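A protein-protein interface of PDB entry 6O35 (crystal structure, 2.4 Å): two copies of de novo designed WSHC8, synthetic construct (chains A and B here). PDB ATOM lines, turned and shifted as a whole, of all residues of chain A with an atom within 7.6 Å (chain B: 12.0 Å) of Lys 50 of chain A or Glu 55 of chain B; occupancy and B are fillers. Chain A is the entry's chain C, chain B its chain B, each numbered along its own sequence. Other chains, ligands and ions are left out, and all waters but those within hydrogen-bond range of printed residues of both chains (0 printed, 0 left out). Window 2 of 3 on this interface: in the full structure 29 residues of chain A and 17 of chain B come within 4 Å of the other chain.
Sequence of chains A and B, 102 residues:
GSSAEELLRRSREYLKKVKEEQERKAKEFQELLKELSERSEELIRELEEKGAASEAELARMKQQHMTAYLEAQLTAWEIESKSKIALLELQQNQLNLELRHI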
ATOM      1  N   LEU A  43     -17.796 -10.380  25.985  1.00  0.00           N
ATOM      2  CA  LEU A  43     -16.570 -11.166  26.055  1.00  0.00           C
ATOM      3  C   LEU A  43     -16.709 -12.306  27.057  1.00  0.00           C
ATOM      4  O   LEU A  43     -16.431 -13.469  26.737  1.00  0.00           O
ATOM      5  CB  LEU A  43     -15.394 -10.266  26.432  1.00  0.00           C
ATOM      6  CG  LEU A  43     -14.896  -9.285  25.372  1.00  0.00           C
ATOM      7  CD1 LEU A  43     -13.843  -8.356  25.965  1.00  0.00           C
ATOM      8  CD2 LEU A  43     -14.339 -10.028  24.166  1.00  0.00           C
ATOM      9  N   ILE A  44     -17.135 -11.991  28.283  1.00  0.00           N
ATOM     10  CA  ILE A  44     -17.268 -13.018  29.311  1.00  0.00           C
ATOM     11  C   ILE A  44     -18.285 -14.069  28.886  1.00  0.00           C
ATOM     12  O   ILE A  44     -18.083 -15.272  29.097  1.00  0.00           O
ATOM     13  CB  ILE A  44     -17.649 -12.378  30.660  1.00  0.00           C
ATOM     14  N   ARG A  45     -19.397 -13.634  28.290  1.00  0.00           N
ATOM     15  CA  ARG A  45     -20.403 -14.576  27.815  1.00  0.00           C
ATOM     16  C   ARG A  45     -19.818 -15.517  26.768  1.00  0.00           C
ATOM     17  O   ARG A  45     -20.096 -16.722  26.783  1.00  0.00           O
ATOM     18  CB  ARG A  45     -21.601 -13.811  27.251  1.00  0.00           C
ATOM     19  CG  ARG A  45     -22.690 -14.680  26.644  1.00  0.00           C
ATOM     20  CD  ARG A  45     -23.424 -13.929  25.538  1.00  0.00           C
ATOM     21  NE  ARG A  45     -24.379 -14.781  24.836  1.00  0.00           N
ATOM     22  N   GLU A  46     -19.010 -14.985  25.849  1.00  0.00           N
ATOM     23  CA  GLU A  46     -18.396 -15.829  24.829  1.00  0.00           C
ATOM     24  C   GLU A  46     -17.531 -16.913  25.459  1.00  0.00           C
ATOM     25  O   GLU A  46     -17.568 -18.072  25.031  1.00  0.00           O
ATOM     26  CB  GLU A  46     -17.565 -14.976  23.869  1.00  0.00           C
ATOM     27  CG  GLU A  46     -18.358 -14.402  22.710  1.00  0.00           C
ATOM     28  CD  GLU A  46     -17.562 -13.399  21.901  1.00  0.00           C
ATOM     29  OE1 GLU A  46     -16.317 -13.393  22.015  1.00  0.00           O
ATOM     30  OE2 GLU A  46     -18.180 -12.607  21.159  1.00  0.00           O
ATOM     31  N   LEU A  47     -16.743 -16.557  26.477  1.00  0.00           N
ATOM     32  CA  LEU A  47     -15.926 -17.552  27.162  1.00  0.00           C
ATOM     33  C   LEU A  47     -16.793 -18.661  27.746  1.00  0.00           C
ATOM     34  O   LEU A  47     -16.497 -19.852  27.582  1.00  0.00           O
ATOM     35  CB  LEU A  47     -15.100 -16.894  28.265  1.00  0.00           C
ATOM     36  CG  LEU A  47     -14.011 -15.909  27.848  1.00  0.00           C
ATOM     37  CD1 LEU A  47     -13.184 -15.512  29.069  1.00  0.00           C
ATOM     38  CD2 LEU A  47     -13.122 -16.476  26.759  1.00  0.00           C
ATOM     39  N   GLU A  48     -17.871 -18.288  28.440  1.00  0.00           N
ATOM     40  CA  GLU A  48     -18.740 -19.293  29.042  1.00  0.00           C
ATOM     41  C   GLU A  48     -19.320 -20.220  27.981  1.00  0.00           C
ATOM     42  O   GLU A  48     -19.431 -21.431  28.199  1.00  0.00           O
ATOM     43  CB  GLU A  48     -19.853 -18.614  29.837  1.00  0.00           C
ATOM     44  CG  GLU A  48     -20.213 -19.339  31.122  1.00  0.00           C
ATOM     45  CD  GLU A  48     -21.373 -18.694  31.853  1.00  0.00           C
ATOM     46  OE1 GLU A  48     -21.935 -17.711  31.327  1.00  0.00           O
ATOM     47  OE2 GLU A  48     -21.723 -19.174  32.952  1.00  0.00           O
ATOM     48  N   GLU A  49     -19.696 -19.669  26.822  1.00  0.00           N
ATOM     49  CA  GLU A  49     -20.124 -20.514  25.712  1.00  0.00           C
ATOM     50  C   GLU A  49     -18.985 -21.413  25.251  1.00  0.00           C
ATOM     51  O   GLU A  49     -19.128 -22.642  25.200  1.00  0.00           O
ATOM     52  CB  GLU A  49     -20.635 -19.654  24.554  1.00  0.00           C
ATOM     53  CG  GLU A  49     -22.098 -19.249  24.671  1.00  0.00           C
ATOM     54  CD  GLU A  49     -22.678 -18.755  23.355  1.00  0.00           C
ATOM     55  OE1 GLU A  49     -22.112 -19.081  22.290  1.00  0.00           O
ATOM     56  OE2 GLU A  49     -23.702 -18.041  23.387  1.00  0.00           O
ATOM     57  N   LYS A  50     -17.838 -20.817  24.916  1.00  0.00           N
ATOM     58  CA  LYS A  50     -16.669 -21.614  24.575  1.00  0.00           C
ATOM     59  C   LYS A  50     -16.271 -22.537  25.717  1.00  0.00           C
ATOM     60  O   LYS A  50     -15.667 -23.591  25.485  1.00  0.00           O
ATOM     61  CB  LYS A  50     -15.485 -20.710  24.229  1.00  0.00           C
ATOM     62  CG  LYS A  50     -15.645 -19.847  22.990  1.00  0.00           C
ATOM     63  CD  LYS A  50     -14.331 -19.124  22.705  1.00  0.00           C
ATOM     64  CE  LYS A  50     -14.534 -17.809  21.971  1.00  0.00           C
ATOM     65  NZ  LYS A  50     -13.502 -16.806  22.373  1.00  0.00           N
ATOM     66  N   GLY A  51     -16.593 -22.162  26.953  1.00  0.00           N
ATOM     67  CA  GLY A  51     -16.032 -22.855  28.093  1.00  0.00           C
ATOM     68  C   GLY A  51     -14.531 -22.734  28.181  1.00  0.00           C
ATOM     69  O   GLY A  51     -13.889 -23.532  28.869  1.00  0.00           O
ATOM     70  N   ALA A  52     -13.950 -21.749  27.492  1.00  0.00           N
ATOM     71  CA  ALA A  52     -12.501 -21.605  27.470  1.00  0.00           C
ATOM     72  C   ALA A  52     -11.953 -21.304  28.857  1.00  0.00           C
ATOM     73  O   ALA A  52     -10.894 -21.815  29.239  1.00  0.00           O
ATOM     74  CB  ALA A  52     -12.105 -20.504  26.487  1.00  0.00           C
ATOM     75  N   ALA A  53     -12.660 -20.481  29.624  1.00  0.00           N
ATOM     76  CA  ALA A  53     -12.200 -20.066  30.940  1.00  0.00           C
ATOM     77  C   ALA A  53     -12.680 -21.032  32.013  1.00  0.00           C
ATOM     78  O   ALA A  53     -13.835 -21.469  32.007  1.00  0.00           O
ATOM     79  CB  ALA A  53     -12.690 -18.650  31.255  1.00  0.00           C
ATOM     80  N   MET A  61     -13.207 -13.290  36.796  1.00  0.00           N
ATOM     81  CA  MET A  61     -13.384 -12.303  35.736  1.00  0.00           C
ATOM     82  C   MET A  61     -14.688 -11.538  35.918  1.00  0.00           C
ATOM     83  O   MET A  61     -14.714 -10.304  35.841  1.00  0.00           O
ATOM     84  CB  MET A  61     -13.349 -12.998  34.375  1.00  0.00           C
ATOM     85  CG  MET A  61     -13.527 -12.064  33.195  1.00  0.00           C
ATOM     86  SD  MET A  61     -13.114 -12.851  31.624  1.00  0.00           S
ATOM     87  CE  MET A  61     -11.395 -13.288  31.891  1.00  0.00           C
ATOM     88  N   ILE B  44      -3.943  -5.535  20.288  1.00  0.00           N
ATOM     89  CA  ILE B  44      -4.827  -6.654  20.596  1.00  0.00           C
ATOM     90  C   ILE B  44      -5.355  -7.294  19.322  1.00  0.00           C
ATOM     91  O   ILE B  44      -5.587  -8.507  19.278  1.00  0.00           O
ATOM     92  CB  ILE B  44      -5.972  -6.183  21.515  1.00  0.00           C
ATOM     93  CG1 ILE B  44      -5.457  -6.034  22.948  1.00  0.00           C
ATOM     94  CG2 ILE B  44      -7.136  -7.152  21.454  1.00  0.00           C
ATOM     95  CD1 ILE B  44      -6.280  -5.102  23.802  1.00  0.00           C
ATOM     96  N   ARG B  45      -5.560  -6.499  18.271  1.00  0.00           N
ATOM     97  CA  ARG B  45      -5.921  -7.071  16.979  1.00  0.00           C
ATOM     98  C   ARG B  45      -4.811  -7.985  16.475  1.00  0.00           C
ATOM     99  O   ARG B  45      -5.061  -9.139  16.106  1.00  0.00           O
ATOM    100  CB  ARG B  45      -6.208  -5.956  15.974  1.00  0.00           C
ATOM    101  CG  ARG B  45      -7.053  -6.390  14.788  1.00  0.00           C
ATOM    102  N   GLU B  46      -3.571  -7.486  16.469  1.00  0.00           N
ATOM    103  CA  GLU B  46      -2.434  -8.302  16.058  1.00  0.00           C
ATOM    104  C   GLU B  46      -2.393  -9.616  16.828  1.00  0.00           C
ATOM    105  O   GLU B  46      -2.235 -10.692  16.238  1.00  0.00           O
ATOM    106  CB  GLU B  46      -1.130  -7.525  16.261  1.00  0.00           C
ATOM    107  CG  GLU B  46      -0.809  -6.528  15.159  1.00  0.00           C
ATOM    108  CD  GLU B  46       0.446  -5.717  15.446  1.00  0.00           C
ATOM    109  OE1 GLU B  46       1.035  -5.887  16.534  1.00  0.00           O
ATOM    110  OE2 GLU B  46       0.841  -4.907  14.581  1.00  0.00           O
ATOM    111  N   LEU B  47      -2.530  -9.548  18.156  1.00  0.00           N
ATOM    112  CA  LEU B  47      -2.500 -10.764  18.960  1.00  0.00           C
ATOM    113  C   LEU B  47      -3.619 -11.718  18.556  1.00  0.00           C
ATOM    114  O   LEU B  47      -3.413 -12.935  18.487  1.00  0.00           O
ATOM    115  CB  LEU B  47      -2.610 -10.423  20.445  1.00  0.00           C
ATOM    116  CG  LEU B  47      -1.406  -9.764  21.114  1.00  0.00           C
ATOM    117  CD1 LEU B  47      -1.671  -9.596  22.608  1.00  0.00           C
ATOM    118  CD2 LEU B  47      -0.131 -10.554  20.890  1.00  0.00           C
ATOM    119  N   GLU B  48      -4.812 -11.185  18.287  1.00  0.00           N
ATOM    120  CA  GLU B  48      -5.934 -12.035  17.906  1.00  0.00           C
ATOM    121  C   GLU B  48      -5.645 -12.770  16.602  1.00  0.00           C
ATOM    122  O   GLU B  48      -5.856 -13.985  16.499  1.00  0.00           O
ATOM    123  CB  GLU B  48      -7.206 -11.195  17.783  1.00  0.00           C
ATOM    124  N   GLU B  49      -5.155 -12.049  15.589  1.00  0.00           N
ATOM    125  CA  GLU B  49      -4.908 -12.675  14.294  1.00  0.00           C
ATOM    126  C   GLU B  49      -3.785 -13.700  14.385  1.00  0.00           C
ATOM    127  O   GLU B  49      -3.826 -14.737  13.713  1.00  0.00           O
ATOM    128  CB  GLU B  49      -4.573 -11.611  13.248  1.00  0.00           C
ATOM    129  CG  GLU B  49      -5.427 -10.360  13.349  1.00  0.00           C
ATOM    130  CD  GLU B  49      -5.664  -9.702  12.005  1.00  0.00           C
ATOM    131  OE1 GLU B  49      -4.678  -9.371  11.315  1.00  0.00           O
ATOM    132  OE2 GLU B  49      -6.845  -9.528  11.637  1.00  0.00           O
ATOM    133  N   LYS B  50      -2.769 -13.422  15.204  1.00  0.00           N
ATOM    134  CA  LYS B  50      -1.703 -14.389  15.413  1.00  0.00           C
ATOM    135  C   LYS B  50      -2.145 -15.554  16.286  1.00  0.00           C
ATOM    136  O   LYS B  50      -1.545 -16.631  16.214  1.00  0.00           O
ATOM    137  CB  LYS B  50      -0.493 -13.721  16.069  1.00  0.00           C
ATOM    138  CG  LYS B  50       0.256 -12.742  15.190  1.00  0.00           C
ATOM    139  CD  LYS B  50       1.417 -12.120  15.952  1.00  0.00           C
ATOM    140  CE  LYS B  50       2.055 -10.985  15.169  1.00  0.00           C
ATOM    141  NZ  LYS B  50       3.274 -10.465  15.848  1.00  0.00           N
ATOM    142  N   GLY B  51      -3.173 -15.365  17.105  1.00  0.00           N
ATOM    143  CA  GLY B  51      -3.454 -16.317  18.157  1.00  0.00           C
ATOM    144  C   GLY B  51      -2.235 -16.488  19.040  1.00  0.00           C
ATOM    145  O   GLY B  51      -1.828 -17.611  19.342  1.00  0.00           O
ATOM    146  N   ALA B  52      -1.628 -15.370  19.440  1.00  0.00           N
ATOM    147  CA  ALA B  52      -0.441 -15.379  20.285  1.00  0.00           C
ATOM    148  C   ALA B  52      -0.770 -15.298  21.769  1.00  0.00           C
ATOM    149  O   ALA B  52       0.141 -15.400  22.598  1.00  0.00           O
ATOM    150  CB  ALA B  52       0.482 -14.215  19.906  1.00  0.00           C
ATOM    151  N   ALA B  53      -2.041 -15.114  22.117  1.00  0.00           N
ATOM    152  CA  ALA B  53      -2.492 -15.077  23.499  1.00  0.00           C
ATOM    153  C   ALA B  53      -3.735 -15.948  23.644  1.00  0.00           C
ATOM    154  O   ALA B  53      -4.550 -16.045  22.724  1.00  0.00           O
ATOM    155  CB  ALA B  53      -2.797 -13.644  23.953  1.00  0.00           C
ATOM    156  N   SER B  54      -3.865 -16.583  24.812  1.00  0.00           N
ATOM    157  CA  SER B  54      -5.018 -17.432  25.088  1.00  0.00           C
ATOM    158  C   SER B  54      -6.306 -16.636  24.894  1.00  0.00           C
ATOM    159  O   SER B  54      -6.335 -15.412  24.995  1.00  0.00           O
ATOM    160  CB  SER B  54      -4.946 -17.960  26.523  1.00  0.00           C
ATOM    161  OG  SER B  54      -6.146 -18.620  26.881  1.00  0.00           O
ATOM    162  N   GLU B  55      -7.394 -17.358  24.601  1.00  0.00           N
ATOM    163  CA  GLU B  55      -8.692 -16.696  24.463  1.00  0.00           C
ATOM    164  C   GLU B  55      -9.061 -15.940  25.734  1.00  0.00           C
ATOM    165  O   GLU B  55      -9.534 -14.797  25.676  1.00  0.00           O
ATOM    166  CB  GLU B  55      -9.778 -17.715  24.115  1.00  0.00           C
ATOM    167  CG  GLU B  55      -9.852 -18.057  22.638  1.00  0.00           C
ATOM    168  CD  GLU B  55     -10.469 -16.945  21.807  1.00  0.00           C
ATOM    169  OE1 GLU B  55     -11.261 -16.148  22.356  1.00  0.00           O
ATOM    170  OE2 GLU B  55     -10.166 -16.872  20.597  1.00  0.00           O
ATOM    171  N   ALA B  56      -8.849 -16.562  26.897  1.00  0.00           N
ATOM    172  CA  ALA B  56      -9.141 -15.894  28.160  1.00  0.00           C
ATOM    173  C   ALA B  56      -8.201 -14.717  28.393  1.00  0.00           C
ATOM    174  O   ALA B  56      -8.617 -13.680  28.923  1.00  0.00           O
ATOM    175  CB  ALA B  56      -9.041 -16.891  29.314  1.00  0.00           C
ATOM    176  N   GLU B  57      -6.929 -14.861  28.015  1.00  0.00           N
ATOM    177  CA  GLU B  57      -5.970 -13.780  28.217  1.00  0.00           C
ATOM    178  C   GLU B  57      -6.376 -12.529  27.449  1.00  0.00           C
ATOM    179  O   GLU B  57      -6.310 -11.415  27.983  1.00  0.00           O
ATOM    180  CB  GLU B  57      -4.571 -14.234  27.801  1.00  0.00           C
ATOM    181  CG  GLU B  57      -3.907 -15.174  28.793  1.00  0.00           C
ATOM    182  N   LEU B  58      -6.797 -12.687  26.191  1.00  0.00           N
ATOM    183  CA  LEU B  58      -7.218 -11.525  25.416  1.00  0.00           C
ATOM    184  C   LEU B  58      -8.511 -10.932  25.964  1.00  0.00           C
ATOM    185  O   LEU B  58      -8.757  -9.732  25.800  1.00  0.00           O
ATOM    186  CB  LEU B  58      -7.382 -11.897  23.945  1.00  0.00           C
ATOM    187  CG  LEU B  58      -6.087 -12.140  23.166  1.00  0.00           C
ATOM    188  CD1 LEU B  58      -6.378 -12.313  21.679  1.00  0.00           C
ATOM    189  CD2 LEU B  58      -5.084 -11.013  23.381  1.00  0.00           C
ATOM    190  N   ALA B  59      -9.349 -11.749  26.609  1.00  0.00           N
ATOM    191  CA  ALA B  59     -10.485 -11.200  27.340  1.00  0.00           C
ATOM    192  C   ALA B  59     -10.005 -10.325  28.489  1.00  0.00           C
ATOM    193  O   ALA B  59     -10.558  -9.245  28.736  1.00  0.00           O
ATOM    194  CB  ALA B  59     -11.375 -12.326  27.861  1.00  0.00           C
ATOM    195  N   ARG B  60      -8.964 -10.773  29.195  1.00  0.00           N
ATOM    196  CA  ARG B  60      -8.396  -9.976  30.275  1.00  0.00           C
ATOM    197  C   ARG B  60      -7.715  -8.725  29.736  1.00  0.00           C
ATOM    198  O   ARG B  60      -7.825  -7.648  30.333  1.00  0.00           O
ATOM    199  CB  ARG B  60      -7.407 -10.821  31.078  1.00  0.00           C
ATOM    200  N   MET B  61      -7.008  -8.845  28.611  1.00  0.00           N
ATOM    201  CA  MET B  61      -6.306  -7.691  28.059  1.00  0.00           C
ATOM    202  C   MET B  61      -7.288  -6.659  27.516  1.00  0.00           C
ATOM    203  O   MET B  61      -7.126  -5.457  27.755  1.00  0.00           O
ATOM    204  CB  MET B  61      -5.339  -8.142  26.965  1.00  0.00           C
ATOM    205  CG  MET B  61      -4.014  -7.396  26.972  1.00  0.00           C
ATOM    206  SD  MET B  61      -2.943  -7.837  25.591  1.00  0.00           S
ATOM    207  CE  MET B  61      -2.554  -9.543  25.983  1.00  0.00           C
ATOM    208  N   LYS B  62      -8.314  -7.107  26.787  1.00  0.00           N
ATOM    209  CA  LYS B  62      -9.315  -6.181  26.265  1.00  0.00           C
ATOM    210  C   LYS B  62     -10.027  -5.446  27.394  1.00  0.00           C
ATOM    211  O   LYS B  62     -10.233  -4.229  27.326  1.00  0.00           O
ATOM    212  CB  LYS B  62     -10.331  -6.933  25.404  1.00  0.00           C
ATOM    213  CG  LYS B  62      -9.980  -6.983  23.933  1.00  0.00           C
ATOM    214  CD  LYS B  62     -11.021  -7.760  23.141  1.00  0.00           C
ATOM    215  CE  LYS B  62     -10.359  -8.773  22.217  1.00  0.00           C
ATOM    216  NZ  LYS B  62     -11.348  -9.494  21.372  1.00  0.00           N
ATOM    217  N   GLN B  63     -10.423  -6.176  28.440  1.00  0.00           N
ATOM    218  CA  GLN B  63     -11.134  -5.551  29.550  1.00  0.00           C
ATOM    219  C   GLN B  63     -10.234  -4.589  30.313  1.00  0.00           C
ATOM    220  O   GLN B  63     -10.697  -3.545  30.788  1.00  0.00           O
ATOM    221  CB  GLN B  63     -11.697  -6.628  30.475  1.00  0.00           C
ATOM    222  CG  GLN B  63     -13.102  -7.074  30.093  1.00  0.00           C
ATOM    223  CD  GLN B  63     -13.500  -8.383  30.738  1.00  0.00           C
ATOM    224  OE1 GLN B  63     -14.363  -8.421  31.615  1.00  0.00           O
ATOM    225  NE2 GLN B  63     -12.876  -9.471  30.298  1.00  0.00           N
ATOM    226  N   GLN B  64      -8.946  -4.918  30.443  1.00  0.00           N
ATOM    227  CA  GLN B  64      -8.004  -3.970  31.025  1.00  0.00           C
ATOM    228  C   GLN B  64      -7.865  -2.734  30.145  1.00  0.00           C
ATOM    229  O   GLN B  64      -7.777  -1.608  30.650  1.00  0.00           O
ATOM    230  CB  GLN B  64      -6.642  -4.633  31.227  1.00  0.00           C
ATOM    231  CG  GLN B  64      -5.516  -3.655  31.518  1.00  0.00           C
ATOM    232  N   MET B  66     -10.171  -1.422  28.116  1.00  0.00           N
ATOM    233  CA  MET B  66     -11.364  -0.601  28.278  1.00  0.00           C
ATOM    234  C   MET B  66     -11.433   0.026  29.665  1.00  0.00           C
ATOM    235  O   MET B  66     -11.960   1.134  29.815  1.00  0.00           O
ATOM    236  CB  MET B  66     -12.613  -1.439  28.013  1.00  0.00           C
ATOM    237  CG  MET B  66     -12.817  -1.790  26.550  1.00  0.00           C
ATOM    238  SD  MET B  66     -14.333  -2.722  26.262  1.00  0.00           S
ATOM    239  CE  MET B  66     -13.954  -4.265  27.090  1.00  0.00           C
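The side-chain carboxylate (OE2) of Glu 55 of chain B is in salt-bridge range of the side-chain amino group (NZ) of Lys 50 of chain A, at 3.8 Å.
The side-chain amide nitrogen (NE2) of Gln 63 of chain B is in hydrogen-bond range of the side-chain sulfur (SD) of Met 61 of chain A (3.6 Å).
The side-chain amide nitrogen (NE2) of Gln 63 of chain B lies within hydrogen-bond range of the backbone carbonyl oxygen (O) of Ala 59 of chain B, at 2.8 Å.
The backbone carbonyl oxygen (O) of Leu 47 of chain A lies within hydrogen-bond range of the backbone NH (N) of Ala 52 of chain A.
Lys 62 of chain B touches Leu 43 of chain A.
Ala 59 of chain B touches Leu 47 of chain A (CB to CD1, 3.9 Å).
No residue of chain B comes within 4 Å of Glu 49 of chain A.
Lys 50 of chain A touches just one residue of chain B: Glu 55 (2.3 Å).
No residue of chain B comes within 4 Å of Ala 52 of chain A.
No residue of chain B comes within 4 Å of Ala 53 of chain A.
Of the printed residues of chain A, Ala 59 of chain B touches Leu 47 (3.9 Å).
Of the printed residues of chain A, Lys 62 of chain B touches Leu 43.
Printed residues of chain A within 4 Å of Gln 63 of chain B: Met 61.
The nearest residue of chain B that does not touch Lys 50 of chain A is Ala 56 of chain B (6.5 Å).
The nearest residue of chain A that does not touch Glu 55 of chain B is Leu 47 of chain A (4.1 Å).
Of the 12 printed residues of chain A, 4 touch a printed residue of chain B.
Among the printed residues, 4 pairs touch across the chains.
Positions printed for both chains: 44, 45, 46, 47, 48, 49, 50, 51, 52, 53 and 61.
Of the 4 pairs that touch across the chains among the printed residues, none has its exchanged pair printed and touching as well.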
